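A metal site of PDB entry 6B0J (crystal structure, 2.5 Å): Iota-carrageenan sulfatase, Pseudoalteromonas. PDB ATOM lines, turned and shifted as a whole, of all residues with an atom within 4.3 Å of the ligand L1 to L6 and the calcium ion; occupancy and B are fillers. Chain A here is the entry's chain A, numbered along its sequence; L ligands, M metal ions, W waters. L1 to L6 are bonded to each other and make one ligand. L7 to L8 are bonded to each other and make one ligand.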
ATOM      1  N   ASP A  11      -3.255  -1.969 -13.143  1.00  0.00           N
ATOM      2  CA  ASP A  11      -3.946  -2.515 -14.306  1.00  0.00           C
ATOM      3  C   ASP A  11      -2.947  -2.849 -15.417  1.00  0.00           C
ATOM      4  O   ASP A  11      -2.352  -1.945 -15.996  1.00  0.00           O
ATOM      5  CB  ASP A  11      -4.967  -1.455 -14.776  1.00  0.00           C
ATOM      6  CG  ASP A  11      -5.914  -1.948 -15.849  1.00  0.00           C
ATOM      7  OD1 ASP A  11      -5.712  -3.034 -16.417  1.00  0.00           O
ATOM      8  OD2 ASP A  11      -6.881  -1.214 -16.149  1.00  0.00           O
ATOM      9  N   ASP A  12      -2.777  -4.144 -15.694  1.00  0.00           N
ATOM     10  CA  ASP A  12      -1.779  -4.667 -16.649  1.00  0.00           C
ATOM     11  C   ASP A  12      -0.321  -4.476 -16.178  1.00  0.00           C
ATOM     12  O   ASP A  12       0.612  -4.428 -17.010  1.00  0.00           O
ATOM     13  CB  ASP A  12      -1.950  -4.086 -18.079  1.00  0.00           C
ATOM     14  CG  ASP A  12      -3.217  -4.559 -18.786  1.00  0.00           C
ATOM     15  OD1 ASP A  12      -3.979  -5.388 -18.237  1.00  0.00           O
ATOM     16  OD2 ASP A  12      -3.458  -4.115 -19.920  1.00  0.00           O
ATOM     17  N   PRO A  49      -7.057 -14.202 -16.337  1.00  0.00           N
ATOM     18  CA  PRO A  49      -5.929 -13.456 -16.902  1.00  0.00           C
ATOM     19  C   PRO A  49      -6.254 -12.127 -17.598  1.00  0.00           C
ATOM     20  O   PRO A  49      -5.432 -11.616 -18.353  1.00  0.00           O
ATOM     21  CB  PRO A  49      -5.309 -14.459 -17.875  1.00  0.00           C
ATOM     22  CG  PRO A  49      -6.465 -15.293 -18.333  1.00  0.00           C
ATOM     23  CD  PRO A  49      -7.359 -15.413 -17.124  1.00  0.00           C
ATOM     24  N   PHE A  50      -7.437 -11.561 -17.339  1.00  0.00           N
ATOM     25  CA  PHE A  50      -7.719 -10.168 -17.722  1.00  0.00           C
ATOM     26  C   PHE A  50      -8.785  -9.509 -16.838  1.00  0.00           C
ATOM     27  O   PHE A  50      -9.376 -10.160 -15.980  1.00  0.00           O
ATOM     28  CB  PHE A  50      -7.980 -10.013 -19.226  1.00  0.00           C
ATOM     29  CG  PHE A  50      -9.156 -10.779 -19.765  1.00  0.00           C
ATOM     30  CD1 PHE A  50     -10.437 -10.326 -19.558  1.00  0.00           C
ATOM     31  CD2 PHE A  50      -8.969 -11.912 -20.549  1.00  0.00           C
ATOM     32  CE1 PHE A  50     -11.531 -10.998 -20.077  1.00  0.00           C
ATOM     33  CE2 PHE A  50     -10.052 -12.609 -21.084  1.00  0.00           C
ATOM     34  CZ  PHE A  50     -11.347 -12.159 -20.838  1.00  0.00           C
ATOM     35  N   SER A  51      -9.011  -8.211 -17.073  1.00  0.00           N
ATOM     36  CA  SER A  51      -9.558  -7.264 -16.088  1.00  0.00           C
ATOM     37  C   SER A  51     -10.900  -7.537 -15.438  1.00  0.00           C
ATOM     38  O   SER A  51     -10.978  -7.679 -14.215  1.00  0.00           O
ATOM     39  CB  SER A  51      -9.650  -5.889 -16.741  1.00  0.00           C
ATOM     40  OG  SER A  51     -10.212  -4.938 -15.877  1.00  0.00           O
ATOM     41  N   ASN A  72     -14.994  -9.606 -20.395  1.00  0.00           N
ATOM     42  CA  ASN A  72     -15.092  -8.172 -20.162  1.00  0.00           C
ATOM     43  C   ASN A  72     -16.450  -7.675 -20.655  1.00  0.00           C
ATOM     44  O   ASN A  72     -17.001  -8.217 -21.628  1.00  0.00           O
ATOM     45  CB  ASN A  72     -13.990  -7.404 -20.889  1.00  0.00           C
ATOM     46  CG  ASN A  72     -12.634  -7.507 -20.215  1.00  0.00           C
ATOM     47  OD1 ASN A  72     -12.523  -7.890 -19.052  1.00  0.00           O
ATOM     48  ND2 ASN A  72     -11.574  -7.147 -20.945  1.00  0.00           N
ATOM     49  N   LYS A 105     -10.827   2.871 -11.679  1.00  0.00           N
ATOM     50  CA  LYS A 105     -11.448   1.923 -12.606  1.00  0.00           C
ATOM     51  C   LYS A 105     -12.449   1.021 -11.907  1.00  0.00           C
ATOM     52  O   LYS A 105     -12.145   0.465 -10.857  1.00  0.00           O
ATOM     53  CB  LYS A 105     -10.370   1.063 -13.271  1.00  0.00           C
ATOM     54  CG  LYS A 105     -10.888   0.070 -14.283  1.00  0.00           C
ATOM     55  CD  LYS A 105      -9.764  -0.493 -15.143  1.00  0.00           C
ATOM     56  CE  LYS A 105     -10.223  -1.761 -15.838  1.00  0.00           C
ATOM     57  NZ  LYS A 105      -9.232  -2.308 -16.792  1.00  0.00           N
ATOM     58  N   HIS A 107     -15.238  -1.156 -14.102  1.00  0.00           N
ATOM     59  CA  HIS A 107     -15.293  -2.283 -15.067  1.00  0.00           C
ATOM     60  C   HIS A 107     -16.170  -3.440 -14.579  1.00  0.00           C
ATOM     61  O   HIS A 107     -15.917  -4.604 -14.900  1.00  0.00           O
ATOM     62  CB  HIS A 107     -13.857  -2.756 -15.402  1.00  0.00           C
ATOM     63  CG  HIS A 107     -13.699  -3.286 -16.800  1.00  0.00           C
ATOM     64  ND1 HIS A 107     -12.645  -4.111 -17.156  1.00  0.00           N
ATOM     65  CD2 HIS A 107     -14.437  -3.106 -17.925  1.00  0.00           C
ATOM     66  CE1 HIS A 107     -12.745  -4.413 -18.440  1.00  0.00           C
ATOM     67  NE2 HIS A 107     -13.814  -3.811 -18.931  1.00  0.00           N
ATOM     68  N   GLY A 130     -13.555   0.339 -18.830  1.00  0.00           N
ATOM     69  CA  GLY A 130     -12.343  -0.478 -18.859  1.00  0.00           C
ATOM     70  C   GLY A 130     -11.025   0.268 -18.766  1.00  0.00           C
ATOM     71  O   GLY A 130      -9.966  -0.331 -18.602  1.00  0.00           O
ATOM     72  N   GLY A 131     -11.091   1.595 -18.885  1.00  0.00           N
ATOM     73  CA  GLY A 131      -9.912   2.431 -18.756  1.00  0.00           C
ATOM     74  C   GLY A 131     -10.254   3.871 -19.053  1.00  0.00           C
ATOM     75  O   GLY A 131     -11.437   4.250 -19.125  1.00  0.00           O
ATOM     76  N   PHE A 155     -16.736   6.976 -26.893  1.00  0.00           N
ATOM     77  CA  PHE A 155     -15.685   6.133 -26.356  1.00  0.00           C
ATOM     78  C   PHE A 155     -15.460   6.455 -24.879  1.00  0.00           C
ATOM     79  O   PHE A 155     -15.183   7.606 -24.531  1.00  0.00           O
ATOM     80  CB  PHE A 155     -14.407   6.365 -27.177  1.00  0.00           C
ATOM     81  CG  PHE A 155     -13.229   5.526 -26.767  1.00  0.00           C
ATOM     82  CD1 PHE A 155     -13.385   4.178 -26.388  1.00  0.00           C
ATOM     83  CD2 PHE A 155     -11.954   6.068 -26.805  1.00  0.00           C
ATOM     84  CE1 PHE A 155     -12.288   3.416 -26.040  1.00  0.00           C
ATOM     85  CE2 PHE A 155     -10.848   5.308 -26.454  1.00  0.00           C
ATOM     86  CZ  PHE A 155     -11.015   3.985 -26.059  1.00  0.00           C
ATOM     87  N   TYR A 157     -13.277   6.105 -22.700  1.00  0.00           N
ATOM     88  CA  TYR A 157     -11.971   6.626 -22.271  1.00  0.00           C
ATOM     89  C   TYR A 157     -11.834   8.161 -22.257  1.00  0.00           C
ATOM     90  O   TYR A 157     -10.909   8.679 -21.616  1.00  0.00           O
ATOM     91  CB  TYR A 157     -10.839   6.059 -23.151  1.00  0.00           C
ATOM     92  CG  TYR A 157     -10.367   4.661 -22.784  1.00  0.00           C
ATOM     93  CD1 TYR A 157      -9.014   4.419 -22.503  1.00  0.00           C
ATOM     94  CD2 TYR A 157     -11.257   3.586 -22.729  1.00  0.00           C
ATOM     95  CE1 TYR A 157      -8.567   3.152 -22.177  1.00  0.00           C
ATOM     96  CE2 TYR A 157     -10.823   2.314 -22.397  1.00  0.00           C
ATOM     97  CZ  TYR A 157      -9.484   2.101 -22.121  1.00  0.00           C
ATOM     98  OH  TYR A 157      -9.031   0.845 -21.789  1.00  0.00           O
ATOM     99  N   HIS A 206      -2.057   0.537 -17.856  1.00  0.00           N
ATOM    100  CA  HIS A 206      -2.860   0.082 -18.998  1.00  0.00           C
ATOM    101  C   HIS A 206      -2.844   1.138 -20.094  1.00  0.00           C
ATOM    102  O   HIS A 206      -2.689   2.325 -19.820  1.00  0.00           O
ATOM    103  CB  HIS A 206      -4.310  -0.144 -18.535  1.00  0.00           C
ATOM    104  CG  HIS A 206      -5.201  -0.797 -19.547  1.00  0.00           C
ATOM    105  ND1 HIS A 206      -5.710  -0.133 -20.627  1.00  0.00           N
ATOM    106  CD2 HIS A 206      -5.739  -2.039 -19.572  1.00  0.00           C
ATOM    107  CE1 HIS A 206      -6.494  -0.941 -21.314  1.00  0.00           C
ATOM    108  NE2 HIS A 206      -6.531  -2.111 -20.695  1.00  0.00           N
ATOM    109  N   THR A 207      -3.022   0.686 -21.339  1.00  0.00           N
ATOM    110  CA  THR A 207      -3.131   1.572 -22.501  1.00  0.00           C
ATOM    111  C   THR A 207      -4.235   2.638 -22.309  1.00  0.00           C
ATOM    112  O   THR A 207      -5.193   2.391 -21.570  1.00  0.00           O
ATOM    113  CB  THR A 207      -3.441   0.769 -23.776  1.00  0.00           C
ATOM    114  OG1 THR A 207      -4.617  -0.012 -23.561  1.00  0.00           O
ATOM    115  CG2 THR A 207      -2.295  -0.166 -24.143  1.00  0.00           C
ATOM    116  N   ASP A 264      -4.175  -6.603 -11.538  1.00  0.00           N
ATOM    117  CA  ASP A 264      -5.398  -7.332 -11.893  1.00  0.00           C
ATOM    118  C   ASP A 264      -5.096  -8.521 -12.794  1.00  0.00           C
ATOM    119  O   ASP A 264      -5.827  -9.506 -12.787  1.00  0.00           O
ATOM    120  CB  ASP A 264      -6.470  -6.412 -12.509  1.00  0.00           C
ATOM    121  CG  ASP A 264      -6.119  -5.896 -13.886  1.00  0.00           C
ATOM    122  OD1 ASP A 264      -4.932  -5.875 -14.301  1.00  0.00           O
ATOM    123  OD2 ASP A 264      -7.065  -5.467 -14.573  1.00  0.00           O
ATOM    124  N   ASN A 265      -4.036  -8.411 -13.594  1.00  0.00           N
ATOM    125  CA  ASN A 265      -3.587  -9.492 -14.453  1.00  0.00           C
ATOM    126  C   ASN A 265      -2.126  -9.269 -14.849  1.00  0.00           C
ATOM    127  O   ASN A 265      -1.486  -8.280 -14.457  1.00  0.00           O
ATOM    128  CB  ASN A 265      -4.502  -9.609 -15.667  1.00  0.00           C
ATOM    129  CG  ASN A 265      -4.664  -8.305 -16.415  1.00  0.00           C
ATOM    130  OD1 ASN A 265      -5.770  -7.741 -16.450  1.00  0.00           O
ATOM    131  ND2 ASN A 265      -3.597  -7.812 -17.024  1.00  0.00           N
ATOM    132  N   LYS A 282      -0.452 -11.009 -20.487  1.00  0.00           N
ATOM    133  CA  LYS A 282      -1.880 -10.720 -20.350  1.00  0.00           C
ATOM    134  C   LYS A 282      -2.777 -11.649 -21.203  1.00  0.00           C
ATOM    135  O   LYS A 282      -2.546 -11.821 -22.401  1.00  0.00           O
ATOM    136  CB  LYS A 282      -2.151  -9.273 -20.766  1.00  0.00           C
ATOM    137  CG  LYS A 282      -3.555  -8.764 -20.454  1.00  0.00           C
ATOM    138  CD  LYS A 282      -3.764  -7.383 -21.049  1.00  0.00           C
ATOM    139  CE  LYS A 282      -5.191  -6.913 -20.864  1.00  0.00           C
ATOM    140  NZ  LYS A 282      -5.411  -5.562 -21.439  1.00  0.00           N
ATOM    141  N   GLY A 283      -3.788 -12.222 -20.552  1.00  0.00           N
ATOM    142  CA  GLY A 283      -4.776 -13.075 -21.210  1.00  0.00           C
ATOM    143  C   GLY A 283      -4.434 -14.557 -21.306  1.00  0.00           C
ATOM    144  O   GLY A 283      -5.317 -15.369 -21.663  1.00  0.00           O
ATOM    145  N   ARG A 360      -9.842 -19.354 -19.483  1.00  0.00           N
ATOM    146  CA  ARG A 360     -10.030 -18.199 -20.352  1.00  0.00           C
ATOM    147  C   ARG A 360     -10.524 -18.687 -21.693  1.00  0.00           C
ATOM    148  O   ARG A 360      -9.872 -19.507 -22.327  1.00  0.00           O
ATOM    149  CB  ARG A 360      -8.715 -17.419 -20.530  1.00  0.00           C
ATOM    150  CG  ARG A 360      -8.819 -16.202 -21.465  1.00  0.00           C
ATOM    151  CD  ARG A 360      -8.339 -16.494 -22.884  1.00  0.00           C
ATOM    152  NE  ARG A 360      -8.792 -15.481 -23.837  1.00  0.00           N
ATOM    153  CZ  ARG A 360      -8.258 -14.267 -24.007  1.00  0.00           C
ATOM    154  NH1 ARG A 360      -8.777 -13.449 -24.899  1.00  0.00           N
ATOM    155  NH2 ARG A 360      -7.209 -13.849 -23.289  1.00  0.00           N
ATOM    156  N   ARG A 362     -11.757 -18.641 -25.724  1.00  0.00           N
ATOM    157  CA  ARG A 362     -11.308 -18.159 -27.021  1.00  0.00           C
ATOM    158  C   ARG A 362     -12.349 -18.600 -28.069  1.00  0.00           C
ATOM    159  O   ARG A 362     -13.449 -19.023 -27.696  1.00  0.00           O
ATOM    160  CB  ARG A 362      -9.895 -18.676 -27.290  1.00  0.00           C
ATOM    161  CG  ARG A 362      -8.855 -18.084 -26.334  1.00  0.00           C
ATOM    162  CD  ARG A 362      -7.426 -18.363 -26.771  1.00  0.00           C
ATOM    163  NE  ARG A 362      -6.443 -17.890 -25.793  1.00  0.00           N
ATOM    164  CZ  ARG A 362      -5.988 -16.635 -25.656  1.00  0.00           C
ATOM    165  NH1 ARG A 362      -6.453 -15.650 -26.425  1.00  0.00           N
ATOM    166  NH2 ARG A 362      -5.066 -16.360 -24.725  1.00  0.00           N
ATOM    167  N   LYS A 363     -12.037 -18.448 -29.358  1.00  0.00           N
ATOM    168  CA  LYS A 363     -12.990 -18.749 -30.435  1.00  0.00           C
ATOM    169  C   LYS A 363     -13.074 -20.261 -30.654  1.00  0.00           C
ATOM    170  O   LYS A 363     -12.208 -20.856 -31.299  1.00  0.00           O
ATOM    171  CB  LYS A 363     -12.619 -18.030 -31.741  1.00  0.00           C
ATOM    172  CG  LYS A 363     -13.700 -18.120 -32.827  1.00  0.00           C
ATOM    173  CD  LYS A 363     -13.221 -17.624 -34.187  1.00  0.00           C
ATOM    174  CE  LYS A 363     -12.977 -16.119 -34.187  1.00  0.00           C
ATOM    175  NZ  LYS A 363     -12.451 -15.593 -35.482  1.00  0.00           N
ATOM    176  N   HIS A 429     -17.675  -9.169 -24.554  1.00  0.00           N
ATOM    177  CA  HIS A 429     -17.081  -7.821 -24.762  1.00  0.00           C
ATOM    178  C   HIS A 429     -17.395  -7.238 -26.153  1.00  0.00           C
ATOM    179  O   HIS A 429     -17.302  -6.039 -26.347  1.00  0.00           O
ATOM    180  CB  HIS A 429     -15.564  -7.821 -24.446  1.00  0.00           C
ATOM    181  CG  HIS A 429     -14.683  -8.110 -25.617  1.00  0.00           C
ATOM    182  ND1 HIS A 429     -14.586  -9.366 -26.183  1.00  0.00           N
ATOM    183  CD2 HIS A 429     -13.820  -7.323 -26.315  1.00  0.00           C
ATOM    184  CE1 HIS A 429     -13.732  -9.329 -27.190  1.00  0.00           C
ATOM    185  NE2 HIS A 429     -13.238  -8.104 -27.280  1.00  0.00           N
ATOM    186  N   GLU A 433     -18.325 -11.916 -30.680  1.00  0.00           N
ATOM    187  CA  GLU A 433     -17.852 -12.894 -29.711  1.00  0.00           C
ATOM    188  C   GLU A 433     -19.002 -13.771 -29.162  1.00  0.00           C
ATOM    189  O   GLU A 433     -18.868 -14.990 -29.055  1.00  0.00           O
ATOM    190  CB  GLU A 433     -17.140 -12.205 -28.540  1.00  0.00           C
ATOM    191  CG  GLU A 433     -16.334 -13.139 -27.663  1.00  0.00           C
ATOM    192  CD  GLU A 433     -15.496 -12.384 -26.654  1.00  0.00           C
ATOM    193  OE1 GLU A 433     -16.041 -11.457 -26.021  1.00  0.00           O
ATOM    194  OE2 GLU A 433     -14.297 -12.728 -26.490  1.00  0.00           O
HETATM  195  C1  LIG L   1     -11.982   2.076 -30.664  1.00  0.00           C
HETATM  196  C2  LIG L   1     -10.741   1.270 -30.270  1.00  0.00           C
HETATM  197  C3  LIG L   1      -9.911   1.964 -29.196  1.00  0.00           C
HETATM  198  C4  LIG L   1      -9.695   3.457 -29.523  1.00  0.00           C
HETATM  199  C5  LIG L   1     -11.031   4.111 -29.893  1.00  0.00           C
HETATM  200  C6  LIG L   1     -10.896   5.577 -30.250  1.00  0.00           C
HETATM  201  O1  LIG L   1     -12.564   1.451 -31.813  1.00  0.00           O
HETATM  202  O2  LIG L   1     -11.127  -0.002 -29.733  1.00  0.00           O
HETATM  203  O3  LIG L   1      -8.670   1.238 -29.080  1.00  0.00           O
HETATM  204  O4  LIG L   1      -8.742   3.596 -30.569  1.00  0.00           O
HETATM  205  O5  LIG L   1     -11.640   3.421 -30.984  1.00  0.00           O
HETATM  206  O6  LIG L   1     -12.213   6.124 -30.380  1.00  0.00           O
HETATM  207  S1  LIG L   1      -7.310   4.116 -30.291  1.00  0.00           S
HETATM  208  O7  LIG L   1      -6.731   3.506 -29.131  1.00  0.00           O
HETATM  209  O8  LIG L   1      -6.474   3.837 -31.428  1.00  0.00           O
HETATM  210  O9  LIG L   1      -7.400   5.705 -29.984  1.00  0.00           O
HETATM  211  C1  LG2 L   2      -6.824   0.437 -27.732  1.00  0.00           C
HETATM  212  C2  LG2 L   2      -7.554  -1.068 -25.920  1.00  0.00           C
HETATM  213  C3  LG2 L   2      -8.548   0.016 -25.584  1.00  0.00           C
HETATM  214  C4  LG2 L   2      -7.688   1.058 -24.887  1.00  0.00           C
HETATM  215  O1  LG2 L   2      -7.113  -1.837 -24.794  1.00  0.00           O
HETATM  216  O2  LG2 L   2      -9.095   0.481 -26.814  1.00  0.00           O
HETATM  217  O3  LG2 L   2      -6.382   0.877 -25.434  1.00  0.00           O
HETATM  218  C5  LG2 L   2      -6.445  -0.167 -26.396  1.00  0.00           C
HETATM  219  O4  LG2 L   2      -6.835  -0.616 -28.683  1.00  0.00           O
HETATM  220  C6  LG2 L   2      -8.190   1.138 -27.716  1.00  0.00           C
HETATM  221  C1  LG3 L   3      -8.126  -2.730 -24.323  1.00  0.00           C
HETATM  222  C2  LG3 L   3      -7.521  -4.100 -24.085  1.00  0.00           C
HETATM  223  C3  LG3 L   3      -8.587  -5.029 -23.531  1.00  0.00           C
HETATM  224  C4  LG3 L   3      -9.159  -4.455 -22.239  1.00  0.00           C
HETATM  225  C5  LG3 L   3      -9.724  -3.074 -22.603  1.00  0.00           C
HETATM  226  C6  LG3 L   3     -10.362  -2.362 -21.425  1.00  0.00           C
HETATM  227  O1  LG3 L   3      -6.986  -4.606 -25.310  1.00  0.00           O
HETATM  228  O2  LG3 L   3      -8.049  -6.349 -23.316  1.00  0.00           O
HETATM  229  O3  LG3 L   3      -8.187  -4.422 -21.179  1.00  0.00           O
HETATM  230  O4  LG3 L   3      -8.691  -2.248 -23.124  1.00  0.00           O
HETATM  231  O5  LG3 L   3     -10.959  -1.186 -21.951  1.00  0.00           O
HETATM  232  S1  LG3 L   3      -8.518  -5.086 -19.833  1.00  0.00           S
HETATM  233  O6  LG3 L   3      -7.283  -5.072 -18.775  1.00  0.00           O
HETATM  234  O7  LG3 L   3      -8.826  -6.461 -20.046  1.00  0.00           O
HETATM  235  O8  LG3 L   3      -9.642  -4.408 -19.306  1.00  0.00           O
HETATM  236  C1  LG4 L   4      -8.995  -7.372 -23.672  1.00  0.00           C
HETATM  237  C2  LG4 L   4      -8.441  -8.740 -23.284  1.00  0.00           C
HETATM  238  C3  LG4 L   4      -9.281  -9.852 -23.933  1.00  0.00           C
HETATM  239  C4  LG4 L   4      -9.317  -9.682 -25.448  1.00  0.00           C
HETATM  240  C5  LG4 L   4     -10.183  -8.458 -25.488  1.00  0.00           C
HETATM  241  C6  LG4 L   4     -11.273  -8.839 -24.492  1.00  0.00           C
HETATM  242  O1  LG4 L   4      -7.075  -8.767 -23.689  1.00  0.00           O
HETATM  243  O2  LG4 L   4     -10.629  -9.685 -23.510  1.00  0.00           O
HETATM  244  O3  LG4 L   4      -9.945 -10.765 -26.140  1.00  0.00           O
HETATM  245  O4  LG4 L   4      -9.370  -7.361 -25.069  1.00  0.00           O
HETATM  246  O5  LG4 L   4      -4.744  -9.481 -23.464  1.00  0.00           O
HETATM  247  O6  LG4 L   4      -6.288 -10.981 -24.370  1.00  0.00           O
HETATM  248  O7  LG4 L   4      -6.429 -10.542 -21.935  1.00  0.00           O
HETATM  249  S1  LG4 L   4      -6.101  -9.936 -23.397  1.00  0.00           S
HETATM  250  C1  LG5 L   5      -9.704 -10.730 -27.561  1.00  0.00           C
HETATM  251  C2  LG5 L   5      -8.769 -11.872 -27.942  1.00  0.00           C
HETATM  252  C3  LG5 L   5      -8.658 -12.046 -29.454  1.00  0.00           C
HETATM  253  C4  LG5 L   5     -10.064 -12.087 -30.080  1.00  0.00           C
HETATM  254  C5  LG5 L   5     -10.873 -10.858 -29.680  1.00  0.00           C
HETATM  255  C6  LG5 L   5     -12.286 -10.842 -30.288  1.00  0.00           C
HETATM  256  O1  LG5 L   5      -7.457 -11.667 -27.397  1.00  0.00           O
HETATM  257  O2  LG5 L   5      -7.854 -13.213 -29.716  1.00  0.00           O
HETATM  258  O3  LG5 L   5     -10.800 -13.252 -29.655  1.00  0.00           O
HETATM  259  O4  LG5 L   5     -10.958 -10.829 -28.251  1.00  0.00           O
HETATM  260  O5  LG5 L   5     -12.819  -9.516 -30.261  1.00  0.00           O
HETATM  261  S1  LG5 L   5     -11.383 -14.318 -30.622  1.00  0.00           S
HETATM  262  O6  LG5 L   5     -12.784 -14.863 -29.978  1.00  0.00           O
HETATM  263  O7  LG5 L   5     -10.447 -15.418 -30.740  1.00  0.00           O
HETATM  264  O8  LG5 L   5     -11.665 -13.753 -31.901  1.00  0.00           O
HETATM  265  C1  LG6 L   6      -6.665 -14.487 -31.482  1.00  0.00           C
HETATM  266  C2  LG6 L   6      -4.477 -13.566 -32.240  1.00  0.00           C
HETATM  267  C3  LG6 L   6      -5.127 -12.203 -32.112  1.00  0.00           C
HETATM  268  C4  LG6 L   6      -5.926 -12.115 -33.413  1.00  0.00           C
HETATM  269  O1  LG6 L   6      -3.473 -13.636 -33.243  1.00  0.00           O
HETATM  270  O2  LG6 L   6      -5.952 -12.211 -30.925  1.00  0.00           O
HETATM  271  O3  LG6 L   6      -6.296 -13.491 -33.697  1.00  0.00           O
HETATM  272  C5  LG6 L   6      -5.718 -14.334 -32.678  1.00  0.00           C
HETATM  273  O4  LG6 L   6      -6.025 -15.239 -30.450  1.00  0.00           O
HETATM  274  C6  LG6 L   6      -7.105 -13.104 -30.967  1.00  0.00           C
HETATM  275  C1  LG7 L   7      -1.787   5.171 -31.431  1.00  0.00           C
HETATM  276  C2  LG7 L   7      -1.866   3.690 -31.812  1.00  0.00           C
HETATM  277  C3  LG7 L   7      -3.193   3.083 -31.353  1.00  0.00           C
HETATM  278  C4  LG7 L   7      -3.424   3.343 -29.856  1.00  0.00           C
HETATM  279  C5  LG7 L   7      -3.271   4.854 -29.553  1.00  0.00           C
HETATM  280  C6  LG7 L   7      -3.405   5.176 -28.064  1.00  0.00           C
HETATM  281  O1  LG7 L   7      -0.502   5.724 -31.766  1.00  0.00           O
HETATM  282  O2  LG7 L   7      -1.737   3.543 -33.235  1.00  0.00           O
HETATM  283  O3  LG7 L   7      -3.217   1.673 -31.653  1.00  0.00           O
HETATM  284  O4  LG7 L   7      -2.555   2.519 -29.046  1.00  0.00           O
HETATM  285  O5  LG7 L   7      -2.002   5.340 -30.024  1.00  0.00           O
HETATM  286  O6  LG7 L   7      -3.312   6.573 -27.804  1.00  0.00           O
HETATM  287  S1  LG7 L   7      -2.976   1.712 -27.793  1.00  0.00           S
HETATM  288  O7  LG7 L   7      -3.658   0.507 -28.180  1.00  0.00           O
HETATM  289  O8  LG7 L   7      -1.786   1.374 -27.055  1.00  0.00           O
HETATM  290  O9  LG7 L   7      -3.943   2.561 -26.777  1.00  0.00           O
HETATM  291  C1  LG8 L   8      -4.559   1.137 -31.804  1.00  0.00           C
HETATM  292  C2  LG8 L   8      -4.537  -0.404 -31.647  1.00  0.00           C
HETATM  293  C3  LG8 L   8      -5.714  -1.071 -32.371  1.00  0.00           C
HETATM  294  C4  LG8 L   8      -5.709  -0.598 -33.810  1.00  0.00           C
HETATM  295  C5  LG8 L   8      -6.283   0.784 -33.537  1.00  0.00           C
HETATM  296  C6  LG8 L   8      -7.370   0.550 -32.481  1.00  0.00           C
HETATM  297  O1  LG8 L   8      -3.289  -0.954 -32.111  1.00  0.00           O
HETATM  298  O2  LG8 L   8      -6.940  -0.621 -31.781  1.00  0.00           O
HETATM  299  O3  LG8 L   8      -6.483  -1.426 -34.707  1.00  0.00           O
HETATM  300  O4  LG8 L   8      -5.220   1.608 -33.020  1.00  0.00           O
HETATM  301  O5  LG8 L   8      -3.037  -2.595 -30.321  1.00  0.00           O
HETATM  302  O6  LG8 L   8      -1.412  -2.516 -32.021  1.00  0.00           O
HETATM  303  O7  LG8 L   8      -3.627  -3.502 -32.593  1.00  0.00           O
HETATM  304  S1  LG8 L   8      -2.817  -2.376 -31.731  1.00  0.00           S
HETATM  305 CA    CA M   1      -5.924  -5.293 -16.880  1.00  0.00          CA
HETATM  306  O   HOH W   1      -4.499  -4.059 -25.762  1.00  0.00           O
HETATM  307  O   HOH W   2     -13.429 -10.357 -22.878  1.00  0.00           O
HETATM  308  O   HOH W   3     -12.352  -5.355 -23.314  1.00  0.00           O
HETATM  309  O   HOH W   4      -3.875  -8.877 -25.932  1.00  0.00           O
HETATM  310  O   HOH W   5      -5.069  -6.658 -24.099  1.00  0.00           O
HETATM  311  O   HOH W   6     -12.691 -11.993 -24.708  1.00  0.00           O
HETATM  312  O   HOH W   7     -13.327 -14.993 -27.269  1.00  0.00           O
HETATM  313  O   HOH W   8     -10.742 -14.648 -26.568  1.00  0.00           O
HETATM  314  O   HOH W   9     -15.303 -15.608 -30.368  1.00  0.00           O
HETATM  315  O   HOH W  10      -4.958 -12.921 -26.304  1.00  0.00           O
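O of Pro 49 touches O7 of LG4 L4, at 3.9 Å. Phe 50 touches the ligand L1 to L6. CE1 of His 107 touches O8 of LG3 L3, 3.2 Å away. CA of Gly 130 touches O5 of LG3 L3 (3.5 Å). CD2 of Phe 155 touches O6 of LIG L1, at 3.6 Å. CB of Lys 363 touches O7 of LG5 L5, 3.5 Å away. Hydrophobic or aromatic side chains that line the ligand L1 to L6: Phe 50, His 107, Phe 155, Tyr 157, His 206 and His 429. Within 4 Å of the ligand L1 to L6: Asp 11, Asp 12, Pro 49, Phe 50, Ser 51, Asn 72, Lys 105, His 107, Gly 130, Phe 155, Tyr 157, His 206, Thr 207, Asn 265, Lys 282, Gly 283, Arg 360, Lys 363 and His 429. Along chain A the residues within 4 Å of the ligand L1 to L6 span positions 11 to 429.
An oxygen (O4) of LG2 L2 lies within hydrogen-bond range of an oxygen (O2) of LG8 L8 (3.1 Å).
The calcium ion is bound by the side-chain carboxylate (OD1) of Asp 11 (2.3 Å), an oxygen (O6) of LG3 L3 (2.3 Å), the side-chain carboxylate (OD1) of Asp 12 (2.4 Å), the side-chain amide oxygen (OD1) of Asn 265 (2.5 Å), the side-chain carboxylate (OD2) of Asp 264 (2.6 Å) and the side-chain carboxylate (OD1) of Asp 264 (2.8 Å).
The side-chain carboxylate (OD2) of Asp 264 sits close to the side-chain hydroxyl (OG) of Ser 51, at 3.4 Å. The side-chain carboxylate (OD2) of Asp 11 lies within salt-bridge range of the side-chain amino group (NZ) of Lys 105 (2.7 Å). The backbone carbonyl oxygen of Gly 283 sits at hydrogen-bond distance from the guanidinium group of Arg 362, 3.2 Å away. O of Gly 130 lies within hydrogen-bond range of NZ of Lys 105, 2.8 Å away. The backbone carbonyl oxygen (O) of Asn 72 lies within hydrogen-bond range of the backbone NH (N) of His 429 (3.1 Å). OD2 of Asp 12 lies within salt-bridge range of NZ of Lys 282 (2.9 Å). OG of Ser 51 is in hydrogen-bond range of ND1 of His 107, 2.9 Å away. The backbone carbonyl oxygen of Asp 11 lies within hydrogen-bond range of the backbone NH of His 206 (3.1 Å).
Water W7 bridges OE2 of Glu 433 (2.6 Å) and O6 of LG5 L5 (2.8 Å). Water W5 bridges the side-chain amino group of Lys 282 (2.9 Å) and an oxygen (O5) of LG4 L4 (2.9 Å). Water W2 bridges an oxygen (O2) of LG4 L4 (2.9 Å) and the backbone NH of Asn 72 (3.0 Å). Water W10 lies within hydrogen-bond range of O1 of LG5 L5 (3.0 Å) and NH1 of Arg 362 (3.1 Å). Water W6 bridges the side-chain carboxylate (OE2) of Glu 433 (2.5 Å) and an oxygen (O2) of LG4 L4 (3.3 Å). Water W8 lies within hydrogen-bond range of the guanidinium group of Arg 360 (2.8 Å) and an oxygen (O3) of LG5 L5 (3.4 Å).
Residues that only touch the calcium ion: Ser 51.
NE2 of His 429 sits close to O5 of LG5 L5. O8 of LG3 L3 lies within salt-bridge range of NZ of Lys 105 (3.3 Å). The guanidinium group (NH2) of Arg 360 is in salt-bridge range of an oxygen (O6) of LG4 L4 (3.2 Å). A ring nitrogen (NE2) of His 206 lies within hydrogen-bond range of an oxygen (O3) of LG3 L3, at 2.9 Å. The side-chain amino group (NZ) of Lys 282 is in salt-bridge range of an oxygen (O7) of LG3 L3 (3.8 Å). The side-chain hydroxyl of Tyr 157 lies within hydrogen-bond range of an oxygen (O5) of LG3 L3, at 2.8 Å. OG1 of Thr 207 lies within hydrogen-bond range of O3 of LG2 L2 (2.7 Å). An oxygen (O7) of LG3 L3 sits at hydrogen-bond distance from the side-chain amide nitrogen (ND2) of Asn 72. An oxygen (O7) of LG4 L4 lies close to the backbone NH (N) of Gly 283, 3.4 Å away. N of Ser 51 sits close to O7 of LG3 L3 (3.5 Å).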
